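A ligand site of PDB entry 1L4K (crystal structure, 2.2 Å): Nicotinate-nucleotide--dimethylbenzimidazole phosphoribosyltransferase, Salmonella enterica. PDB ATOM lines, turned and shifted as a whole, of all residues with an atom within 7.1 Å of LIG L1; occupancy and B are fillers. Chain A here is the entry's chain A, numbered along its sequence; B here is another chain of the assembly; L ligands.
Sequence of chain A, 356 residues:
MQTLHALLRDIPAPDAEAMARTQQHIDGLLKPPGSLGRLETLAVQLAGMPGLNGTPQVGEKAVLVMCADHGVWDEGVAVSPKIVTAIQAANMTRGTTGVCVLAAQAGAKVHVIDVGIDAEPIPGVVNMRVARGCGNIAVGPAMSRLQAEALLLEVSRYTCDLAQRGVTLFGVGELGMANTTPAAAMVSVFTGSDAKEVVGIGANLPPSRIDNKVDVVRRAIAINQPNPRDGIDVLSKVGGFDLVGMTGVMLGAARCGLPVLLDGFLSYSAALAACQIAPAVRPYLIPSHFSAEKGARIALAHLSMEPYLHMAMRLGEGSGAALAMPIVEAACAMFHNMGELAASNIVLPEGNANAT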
ATOM      1  N   SER A  80      -1.152  22.460  17.924  1.00  0.00           N
ATOM      2  CA  SER A  80      -0.523  22.780  16.641  1.00  0.00           C
ATOM      3  C   SER A  80      -0.643  24.273  16.377  1.00  0.00           C
ATOM      4  O   SER A  80      -1.698  24.867  16.585  1.00  0.00           O
ATOM      5  CB  SER A  80      -1.240  22.051  15.478  1.00  0.00           C
ATOM      6  OG  SER A  80      -0.985  20.662  15.421  1.00  0.00           O
ATOM      7  N   PRO A  81       0.434  24.921  15.914  1.00  0.00           N
ATOM      8  CA  PRO A  81       0.398  26.354  15.622  1.00  0.00           C
ATOM      9  C   PRO A  81      -0.699  26.600  14.567  1.00  0.00           C
ATOM     10  O   PRO A  81      -0.966  25.728  13.746  1.00  0.00           O
ATOM     11  CB  PRO A  81       1.794  26.625  15.070  1.00  0.00           C
ATOM     12  CG  PRO A  81       2.642  25.642  15.822  1.00  0.00           C
ATOM     13  CD  PRO A  81       1.807  24.386  15.758  1.00  0.00           C
ATOM     14  N   VAL A  84      -0.182  26.114  10.627  1.00  0.00           N
ATOM     15  CA  VAL A  84      -0.053  24.785  10.059  1.00  0.00           C
ATOM     16  C   VAL A  84      -1.128  24.546   9.008  1.00  0.00           C
ATOM     17  O   VAL A  84      -0.886  23.860   8.036  1.00  0.00           O
ATOM     18  CB  VAL A  84      -0.074  23.679  11.168  1.00  0.00           C
ATOM     19  CG1 VAL A  84      -0.173  22.292  10.533  1.00  0.00           C
ATOM     20  CG2 VAL A  84       1.230  23.738  11.990  1.00  0.00           C
ATOM     21  N   GLN A  88       0.257  23.361   5.468  1.00  0.00           N
ATOM     22  CA  GLN A  88      -0.145  22.049   4.999  1.00  0.00           C
ATOM     23  C   GLN A  88      -0.965  22.145   3.732  1.00  0.00           C
ATOM     24  O   GLN A  88      -0.861  21.293   2.846  1.00  0.00           O
ATOM     25  CB  GLN A  88      -0.957  21.324   6.065  1.00  0.00           C
ATOM     26  CG  GLN A  88      -0.150  20.348   6.911  1.00  0.00           C
ATOM     27  CD  GLN A  88       0.628  19.329   6.064  1.00  0.00           C
ATOM     28  OE1 GLN A  88       1.656  19.651   5.479  1.00  0.00           O
ATOM     29  NE2 GLN A  88       0.119  18.105   6.017  1.00  0.00           N
ATOM     30  N   ASN A  91       1.421  22.377   1.055  1.00  0.00           N
ATOM     31  CA  ASN A  91       2.065  21.083   0.833  1.00  0.00           C
ATOM     32  C   ASN A  91       1.167  20.144   0.052  1.00  0.00           C
ATOM     33  O   ASN A  91       1.649  19.232  -0.631  1.00  0.00           O
ATOM     34  CB  ASN A  91       2.478  20.426   2.167  1.00  0.00           C
ATOM     35  CG  ASN A  91       3.656  21.125   2.821  1.00  0.00           C
ATOM     36  OD1 ASN A  91       4.458  21.756   2.145  1.00  0.00           O
ATOM     37  ND2 ASN A  91       3.774  20.991   4.135  1.00  0.00           N
ATOM     38  N   MET A  92      -0.136  20.338   0.170  1.00  0.00           N
ATOM     39  CA  MET A  92      -1.090  19.491  -0.542  1.00  0.00           C
ATOM     40  C   MET A  92      -0.907  19.655  -2.050  1.00  0.00           C
ATOM     41  O   MET A  92      -1.094  18.710  -2.804  1.00  0.00           O
ATOM     42  CB  MET A  92      -2.519  19.876  -0.193  1.00  0.00           C
ATOM     43  CG  MET A  92      -2.882  19.750   1.275  1.00  0.00           C
ATOM     44  SD  MET A  92      -3.717  18.211   1.538  1.00  0.00           S
ATOM     45  CE  MET A  92      -4.077  18.318   3.279  1.00  0.00           C
ATOM     46  N   THR A  97       2.000  15.391   1.317  1.00  0.00           N
ATOM     47  CA  THR A  97       1.241  15.052   2.528  1.00  0.00           C
ATOM     48  C   THR A  97       0.713  13.620   2.536  1.00  0.00           C
ATOM     49  O   THR A  97       0.722  12.919   1.513  1.00  0.00           O
ATOM     50  CB  THR A  97       0.017  16.000   2.733  1.00  0.00           C
ATOM     51  OG1 THR A  97      -1.003  15.665   1.779  1.00  0.00           O
ATOM     52  CG2 THR A  97       0.409  17.458   2.569  1.00  0.00           C
ATOM     53  N   GLU A 174     -10.436  16.796   5.321  1.00  0.00           N
ATOM     54  CA  GLU A 174     -10.280  18.176   5.780  1.00  0.00           C
ATOM     55  C   GLU A 174      -8.885  18.473   6.318  1.00  0.00           C
ATOM     56  O   GLU A 174      -8.038  17.594   6.446  1.00  0.00           O
ATOM     57  CB  GLU A 174     -11.297  18.478   6.886  1.00  0.00           C
ATOM     58  CG  GLU A 174     -11.437  17.356   7.929  1.00  0.00           C
ATOM     59  CD  GLU A 174     -10.101  16.940   8.529  1.00  0.00           C
ATOM     60  OE1 GLU A 174      -9.458  17.753   9.209  1.00  0.00           O
ATOM     61  OE2 GLU A 174      -9.689  15.770   8.313  1.00  0.00           O
ATOM     62  N   LEU A 175      -8.695  19.749   6.643  1.00  0.00           N
ATOM     63  CA  LEU A 175      -7.457  20.284   7.196  1.00  0.00           C
ATOM     64  C   LEU A 175      -7.850  21.566   7.927  1.00  0.00           C
ATOM     65  O   LEU A 175      -8.414  22.483   7.323  1.00  0.00           O
ATOM     66  CB  LEU A 175      -6.481  20.610   6.068  1.00  0.00           C
ATOM     67  CG  LEU A 175      -5.126  21.209   6.463  1.00  0.00           C
ATOM     68  CD1 LEU A 175      -4.354  20.169   7.304  1.00  0.00           C
ATOM     69  CD2 LEU A 175      -4.311  21.575   5.204  1.00  0.00           C
ATOM     70  N   GLY A 176      -7.577  21.609   9.229  1.00  0.00           N
ATOM     71  CA  GLY A 176      -7.901  22.779  10.027  1.00  0.00           C
ATOM     72  C   GLY A 176      -7.568  22.584  11.493  1.00  0.00           C
ATOM     73  O   GLY A 176      -8.196  21.788  12.186  1.00  0.00           O
ATOM     74  N   MET A 177      -6.568  23.311  11.973  1.00  0.00           N
ATOM     75  CA  MET A 177      -6.161  23.218  13.356  1.00  0.00           C
ATOM     76  C   MET A 177      -7.329  23.549  14.255  1.00  0.00           C
ATOM     77  O   MET A 177      -8.061  24.520  14.018  1.00  0.00           O
ATOM     78  CB  MET A 177      -4.978  24.151  13.620  1.00  0.00           C
ATOM     79  CG  MET A 177      -3.804  23.942  12.667  1.00  0.00           C
ATOM     80  SD  MET A 177      -3.210  22.232  12.661  1.00  0.00           S
ATOM     81  CE  MET A 177      -3.851  21.643  11.058  1.00  0.00           C
ATOM     82  N   ALA A 203      -5.090  16.237  17.570  1.00  0.00           N
ATOM     83  CA  ALA A 203      -3.708  16.077  17.139  1.00  0.00           C
ATOM     84  C   ALA A 203      -2.730  16.183  18.323  1.00  0.00           C
ATOM     85  O   ALA A 203      -2.061  17.210  18.518  1.00  0.00           O
ATOM     86  CB  ALA A 203      -3.366  17.131  16.064  1.00  0.00           C
ATOM     87  N   ARG A 314      -5.624   8.747  12.822  1.00  0.00           N
ATOM     88  CA  ARG A 314      -6.200   9.997  13.332  1.00  0.00           C
ATOM     89  C   ARG A 314      -5.472  11.197  12.709  1.00  0.00           C
ATOM     90  O   ARG A 314      -5.267  12.217  13.362  1.00  0.00           O
ATOM     91  CB  ARG A 314      -6.057  10.037  14.865  1.00  0.00           C
ATOM     92  CG  ARG A 314      -4.648   9.773  15.369  1.00  0.00           C
ATOM     93  CD  ARG A 314      -4.631   9.623  16.879  1.00  0.00           C
ATOM     94  NE  ARG A 314      -3.329   9.248  17.438  1.00  0.00           N
ATOM     95  CZ  ARG A 314      -2.275  10.061  17.525  1.00  0.00           C
ATOM     96  NH1 ARG A 314      -2.332  11.304  17.081  1.00  0.00           N
ATOM     97  NH2 ARG A 314      -1.155   9.611  18.101  1.00  0.00           N
ATOM     98  N   LEU A 315      -5.082  11.081  11.456  1.00  0.00           N
ATOM     99  CA  LEU A 315      -4.401  12.163  10.769  1.00  0.00           C
ATOM    100  C   LEU A 315      -5.387  13.142  10.132  1.00  0.00           C
ATOM    101  O   LEU A 315      -5.184  14.346  10.195  1.00  0.00           O
ATOM    102  CB  LEU A 315      -3.484  11.597   9.685  1.00  0.00           C
ATOM    103  CG  LEU A 315      -2.899  12.574   8.649  1.00  0.00           C
ATOM    104  CD1 LEU A 315      -2.020  13.628   9.331  1.00  0.00           C
ATOM    105  CD2 LEU A 315      -2.095  11.799   7.612  1.00  0.00           C
ATOM    106  N   GLY A 316      -6.450  12.613   9.536  1.00  0.00           N
ATOM    107  CA  GLY A 316      -7.404  13.455   8.857  1.00  0.00           C
ATOM    108  C   GLY A 316      -6.946  13.560   7.395  1.00  0.00           C
ATOM    109  O   GLY A 316      -6.308  12.621   6.876  1.00  0.00           O
ATOM    110  N   GLU A 317      -7.274  14.666   6.740  1.00  0.00           N
ATOM    111  CA  GLU A 317      -6.890  14.938   5.351  1.00  0.00           C
ATOM    112  C   GLU A 317      -7.611  14.086   4.309  1.00  0.00           C
ATOM    113  O   GLU A 317      -7.499  14.331   3.105  1.00  0.00           O
ATOM    114  CB  GLU A 317      -5.390  14.699   5.147  1.00  0.00           C
ATOM    115  CG  GLU A 317      -4.485  15.541   6.025  1.00  0.00           C
ATOM    116  CD  GLU A 317      -3.019  15.354   5.692  1.00  0.00           C
ATOM    117  OE1 GLU A 317      -2.729  14.693   4.656  1.00  0.00           O
ATOM    118  OE2 GLU A 317      -2.180  15.879   6.443  1.00  0.00           O
ATOM    119  N   LEU B  29       8.051  12.819   9.772  1.00  0.00           N
ATOM    120  CA  LEU B  29       7.245  13.044   8.577  1.00  0.00           C
ATOM    121  C   LEU B  29       6.178  14.117   8.817  1.00  0.00           C
ATOM    122  O   LEU B  29       5.804  14.383   9.959  1.00  0.00           O
ATOM    123  CB  LEU B  29       6.598  11.748   8.112  1.00  0.00           C
ATOM    124  CG  LEU B  29       7.568  10.639   7.745  1.00  0.00           C
ATOM    125  CD1 LEU B  29       6.806   9.369   7.411  1.00  0.00           C
ATOM    126  CD2 LEU B  29       8.435  11.080   6.566  1.00  0.00           C
ATOM    127  N   LEU B  30       5.698  14.701   7.728  1.00  0.00           N
ATOM    128  CA  LEU B  30       4.688  15.760   7.748  1.00  0.00           C
ATOM    129  C   LEU B  30       3.331  15.382   8.354  1.00  0.00           C
ATOM    130  O   LEU B  30       2.322  15.298   7.647  1.00  0.00           O
ATOM    131  CB  LEU B  30       4.487  16.243   6.312  1.00  0.00           C
ATOM    132  CG  LEU B  30       4.408  17.723   5.943  1.00  0.00           C
ATOM    133  CD1 LEU B  30       5.263  18.608   6.828  1.00  0.00           C
ATOM    134  CD2 LEU B  30       4.859  17.810   4.474  1.00  0.00           C
ATOM    135  N   LYS B  31       3.317  15.159   9.661  1.00  0.00           N
ATOM    136  CA  LYS B  31       2.087  14.797  10.348  1.00  0.00           C
ATOM    137  C   LYS B  31       2.342  14.763  11.851  1.00  0.00           C
ATOM    138  O   LYS B  31       3.496  14.736  12.304  1.00  0.00           O
ATOM    139  CB  LYS B  31       1.659  13.394   9.907  1.00  0.00           C
ATOM    140  CG  LYS B  31       2.707  12.338  10.238  1.00  0.00           C
ATOM    141  CD  LYS B  31       2.259  10.934   9.887  1.00  0.00           C
ATOM    142  CE  LYS B  31       3.395   9.940  10.068  1.00  0.00           C
ATOM    143  NZ  LYS B  31       4.051  10.034  11.395  1.00  0.00           N
ATOM    144  N   PRO B  32       1.271  14.763  12.649  1.00  0.00           N
ATOM    145  CA  PRO B  32       1.461  14.709  14.097  1.00  0.00           C
ATOM    146  C   PRO B  32       2.060  13.320  14.371  1.00  0.00           C
ATOM    147  O   PRO B  32       1.658  12.339  13.759  1.00  0.00           O
ATOM    148  CB  PRO B  32       0.027  14.827  14.643  1.00  0.00           C
ATOM    149  CG  PRO B  32      -0.667  15.637  13.576  1.00  0.00           C
ATOM    150  CD  PRO B  32      -0.134  15.040  12.293  1.00  0.00           C
ATOM    151  N   PRO B  33       3.054  13.238  15.263  1.00  0.00           N
ATOM    152  CA  PRO B  33       3.671  11.952  15.584  1.00  0.00           C
ATOM    153  C   PRO B  33       2.641  10.881  15.974  1.00  0.00           C
ATOM    154  O   PRO B  33       1.722  11.148  16.774  1.00  0.00           O
ATOM    155  CB  PRO B  33       4.614  12.293  16.737  1.00  0.00           C
ATOM    156  CG  PRO B  33       5.076  13.682  16.393  1.00  0.00           C
ATOM    157  CD  PRO B  33       3.775  14.353  15.908  1.00  0.00           C
ATOM    158  N   SER B  35       0.184   9.791  14.430  1.00  0.00           N
ATOM    159  CA  SER B  35      -1.151   9.999  13.861  1.00  0.00           C
ATOM    160  C   SER B  35      -1.574   8.977  12.790  1.00  0.00           C
ATOM    161  O   SER B  35      -2.760   8.832  12.526  1.00  0.00           O
ATOM    162  CB  SER B  35      -1.273  11.402  13.281  1.00  0.00           C
ATOM    163  OG  SER B  35      -0.452  11.558  12.145  1.00  0.00           O
ATOM    164  N   LEU B 341       8.603  17.381   8.436  1.00  0.00           N
ATOM    165  CA  LEU B 341       8.259  18.543   9.245  1.00  0.00           C
ATOM    166  C   LEU B 341       9.301  19.647   9.188  1.00  0.00           C
ATOM    167  O   LEU B 341       8.981  20.821   8.936  1.00  0.00           O
ATOM    168  CB  LEU B 341       8.062  18.116  10.702  1.00  0.00           C
ATOM    169  CG  LEU B 341       6.809  17.301  11.047  1.00  0.00           C
ATOM    170  CD1 LEU B 341       6.864  16.777  12.489  1.00  0.00           C
ATOM    171  CD2 LEU B 341       5.578  18.181  10.849  1.00  0.00           C
ATOM    172  N   ILE B 346       7.924  23.345  10.558  1.00  0.00           N
ATOM    173  CA  ILE B 346       6.851  23.096  11.500  1.00  0.00           C
ATOM    174  C   ILE B 346       7.438  22.491  12.766  1.00  0.00           C
ATOM    175  O   ILE B 346       8.113  21.463  12.724  1.00  0.00           O
ATOM    176  CB  ILE B 346       5.778  22.132  10.903  1.00  0.00           C
ATOM    177  CG1 ILE B 346       5.129  22.783   9.684  1.00  0.00           C
ATOM    178  CG2 ILE B 346       4.703  21.828  11.935  1.00  0.00           C
ATOM    179  CD1 ILE B 346       4.136  21.870   8.977  1.00  0.00           C
ATOM    180  N   LEU B 348       6.416  21.110  16.550  1.00  0.00           N
ATOM    181  CA  LEU B 348       5.335  20.681  17.425  1.00  0.00           C
ATOM    182  C   LEU B 348       5.887  20.338  18.808  1.00  0.00           C
ATOM    183  O   LEU B 348       7.022  19.867  18.923  1.00  0.00           O
ATOM    184  CB  LEU B 348       4.632  19.452  16.848  1.00  0.00           C
ATOM    185  CG  LEU B 348       4.164  19.541  15.392  1.00  0.00           C
ATOM    186  CD1 LEU B 348       3.599  18.198  14.956  1.00  0.00           C
ATOM    187  CD2 LEU B 348       3.131  20.635  15.253  1.00  0.00           C
HETATM  188  N1  LIG L   1      -3.134  16.837   8.951  1.00  0.00           N
HETATM  189  C1  LIG L   1      -2.224  17.464   9.872  1.00  0.00           C
HETATM  190  C2  LIG L   1      -2.716  17.882  11.154  1.00  0.00           C
HETATM  191  C3  LIG L   1      -1.882  18.484  12.048  1.00  0.00           C
HETATM  192  C4  LIG L   1      -0.537  18.710  11.743  1.00  0.00           C
HETATM  193  C5  LIG L   1      -0.037  18.303  10.456  1.00  0.00           C
HETATM  194  C6  LIG L   1      -0.915  17.672   9.537  1.00  0.00           C
HETATM  195  C7  LIG L   1       0.373  19.379  12.771  1.00  0.00           C
HETATM  196  C8  LIG L   1       1.422  18.538  10.114  1.00  0.00           C
HETATM  197  P1  LG2 L   2      -6.903  19.371  16.679  1.00  0.00           P
HETATM  198  O1  LG2 L   2      -8.337  19.628  17.004  1.00  0.00           O
HETATM  199  O2  LG2 L   2      -6.153  18.940  17.902  1.00  0.00           O
HETATM  200  O3  LG2 L   2      -6.195  20.720  16.083  1.00  0.00           O
HETATM  201  O4  LG2 L   2      -6.801  18.233  15.566  1.00  0.00           O
HETATM  202  C1  LG2 L   2      -7.476  18.429  14.292  1.00  0.00           C
HETATM  203  C2  LG2 L   2      -6.542  18.352  13.243  1.00  0.00           C
HETATM  204  O5  LG2 L   2      -5.837  17.065  13.271  1.00  0.00           O
HETATM  205  C3  LG2 L   2      -7.126  18.485  11.843  1.00  0.00           C
HETATM  206  O6  LG2 L   2      -6.291  19.251  10.916  1.00  0.00           O
HETATM  207  C4  LG2 L   2      -7.344  16.986  11.435  1.00  0.00           C
HETATM  208  O7  LG2 L   2      -7.018  16.830  10.025  1.00  0.00           O
HETATM  209  C5  LG2 L   2      -6.446  16.164  12.381  1.00  0.00           C
HETATM  210  N1  LG2 L   2      -7.134  15.040  13.157  1.00  0.00           N
HETATM  211  C6  LG2 L   2      -6.921  14.860  14.572  1.00  0.00           C
HETATM  212  C7  LG2 L   2      -7.631  13.772  15.123  1.00  0.00           C
HETATM  213  C8  LG2 L   2      -8.497  12.871  14.418  1.00  0.00           C
HETATM  214  C9  LG2 L   2      -8.608  13.182  12.993  1.00  0.00           C
HETATM  215  C10 LG2 L   2      -7.942  14.242  12.385  1.00  0.00           C
HETATM  216  C11 LG2 L   2      -9.552  12.149  12.397  1.00  0.00           C
HETATM  217  O8  LG2 L   2     -10.116  11.243  12.967  1.00  0.00           O
HETATM  218  O9  LG2 L   2      -9.674  12.402  11.080  1.00  0.00           O
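OE2 of Glu 317 sits at hydrogen-bond distance from N1 of LIG L1. The backbone carbonyl oxygen (O) of Leu 315 lies close to a nitrogen (N1) of LIG L1 (3.5 Å). O of Leu 315 is in hydrogen-bond range of O7 of LG2 L2, 3.1 Å away. N of Ala 203 is in hydrogen-bond range of O2 of LG2 L2, at 2.9 Å. An oxygen (O7) of LG2 L2 is in hydrogen-bond range of the side-chain carboxylate (OE1) of Glu 174 (2.7 Å). O6 of LG2 L2 is in hydrogen-bond range of N of Gly 176 (3.2 Å). The backbone carbonyl oxygen of Gly 176 is in hydrogen-bond range of an oxygen (O6) of LG2 L2, at 3.4 Å.
The side-chain carboxylate (OE2) of Glu 317 sits at hydrogen-bond distance from the side-chain amide nitrogen (NE2) of Gln 88 (3.2 Å). The backbone NH (N) of Glu 317 is in hydrogen-bond range of the backbone carbonyl oxygen (O) of Glu 174 (3.0 Å). The side-chain hydroxyl (OG1) of Thr 97 lies within hydrogen-bond range of the side-chain carboxylate (OE1) of Glu 317, 3.5 Å away. O of Ser 35 of chain B lies within hydrogen-bond range of N of Leu 315 (3.4 Å). The backbone carbonyl oxygen of Pro 32 of chain B is in hydrogen-bond range of the side-chain hydroxyl of Ser 35 of chain B (2.8 Å). OE1 of Gln 88 lies within hydrogen-bond range of ND2 of Asn 91 (2.8 Å).
Ser 80 touches LIG L1. Val 84 touches LIG L1. Gln 88 touches LIG L1. Leu 175 touches LIG L1. Met 177 touches LIG L1 (CE to C3, 3.9 Å). Lys 31 of chain B touches LIG L1 (CA to C8, 3.8 Å). Pro 32 of chain B touches LIG L1 (CG to C3, 3.5 Å). Leu 348 of chain B touches LIG L1. Hydrophobic or aromatic side chains within 4 Å of LIG L1: Val 84, Leu 175, Met 177, Leu 315, Pro 32 of chain B and Leu 348 of chain B. Of the 25 residues printed, 10 come within 4 Å of LIG L1. Along chain A the residues within 4 Å of LIG L1 span positions 80 to 317.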
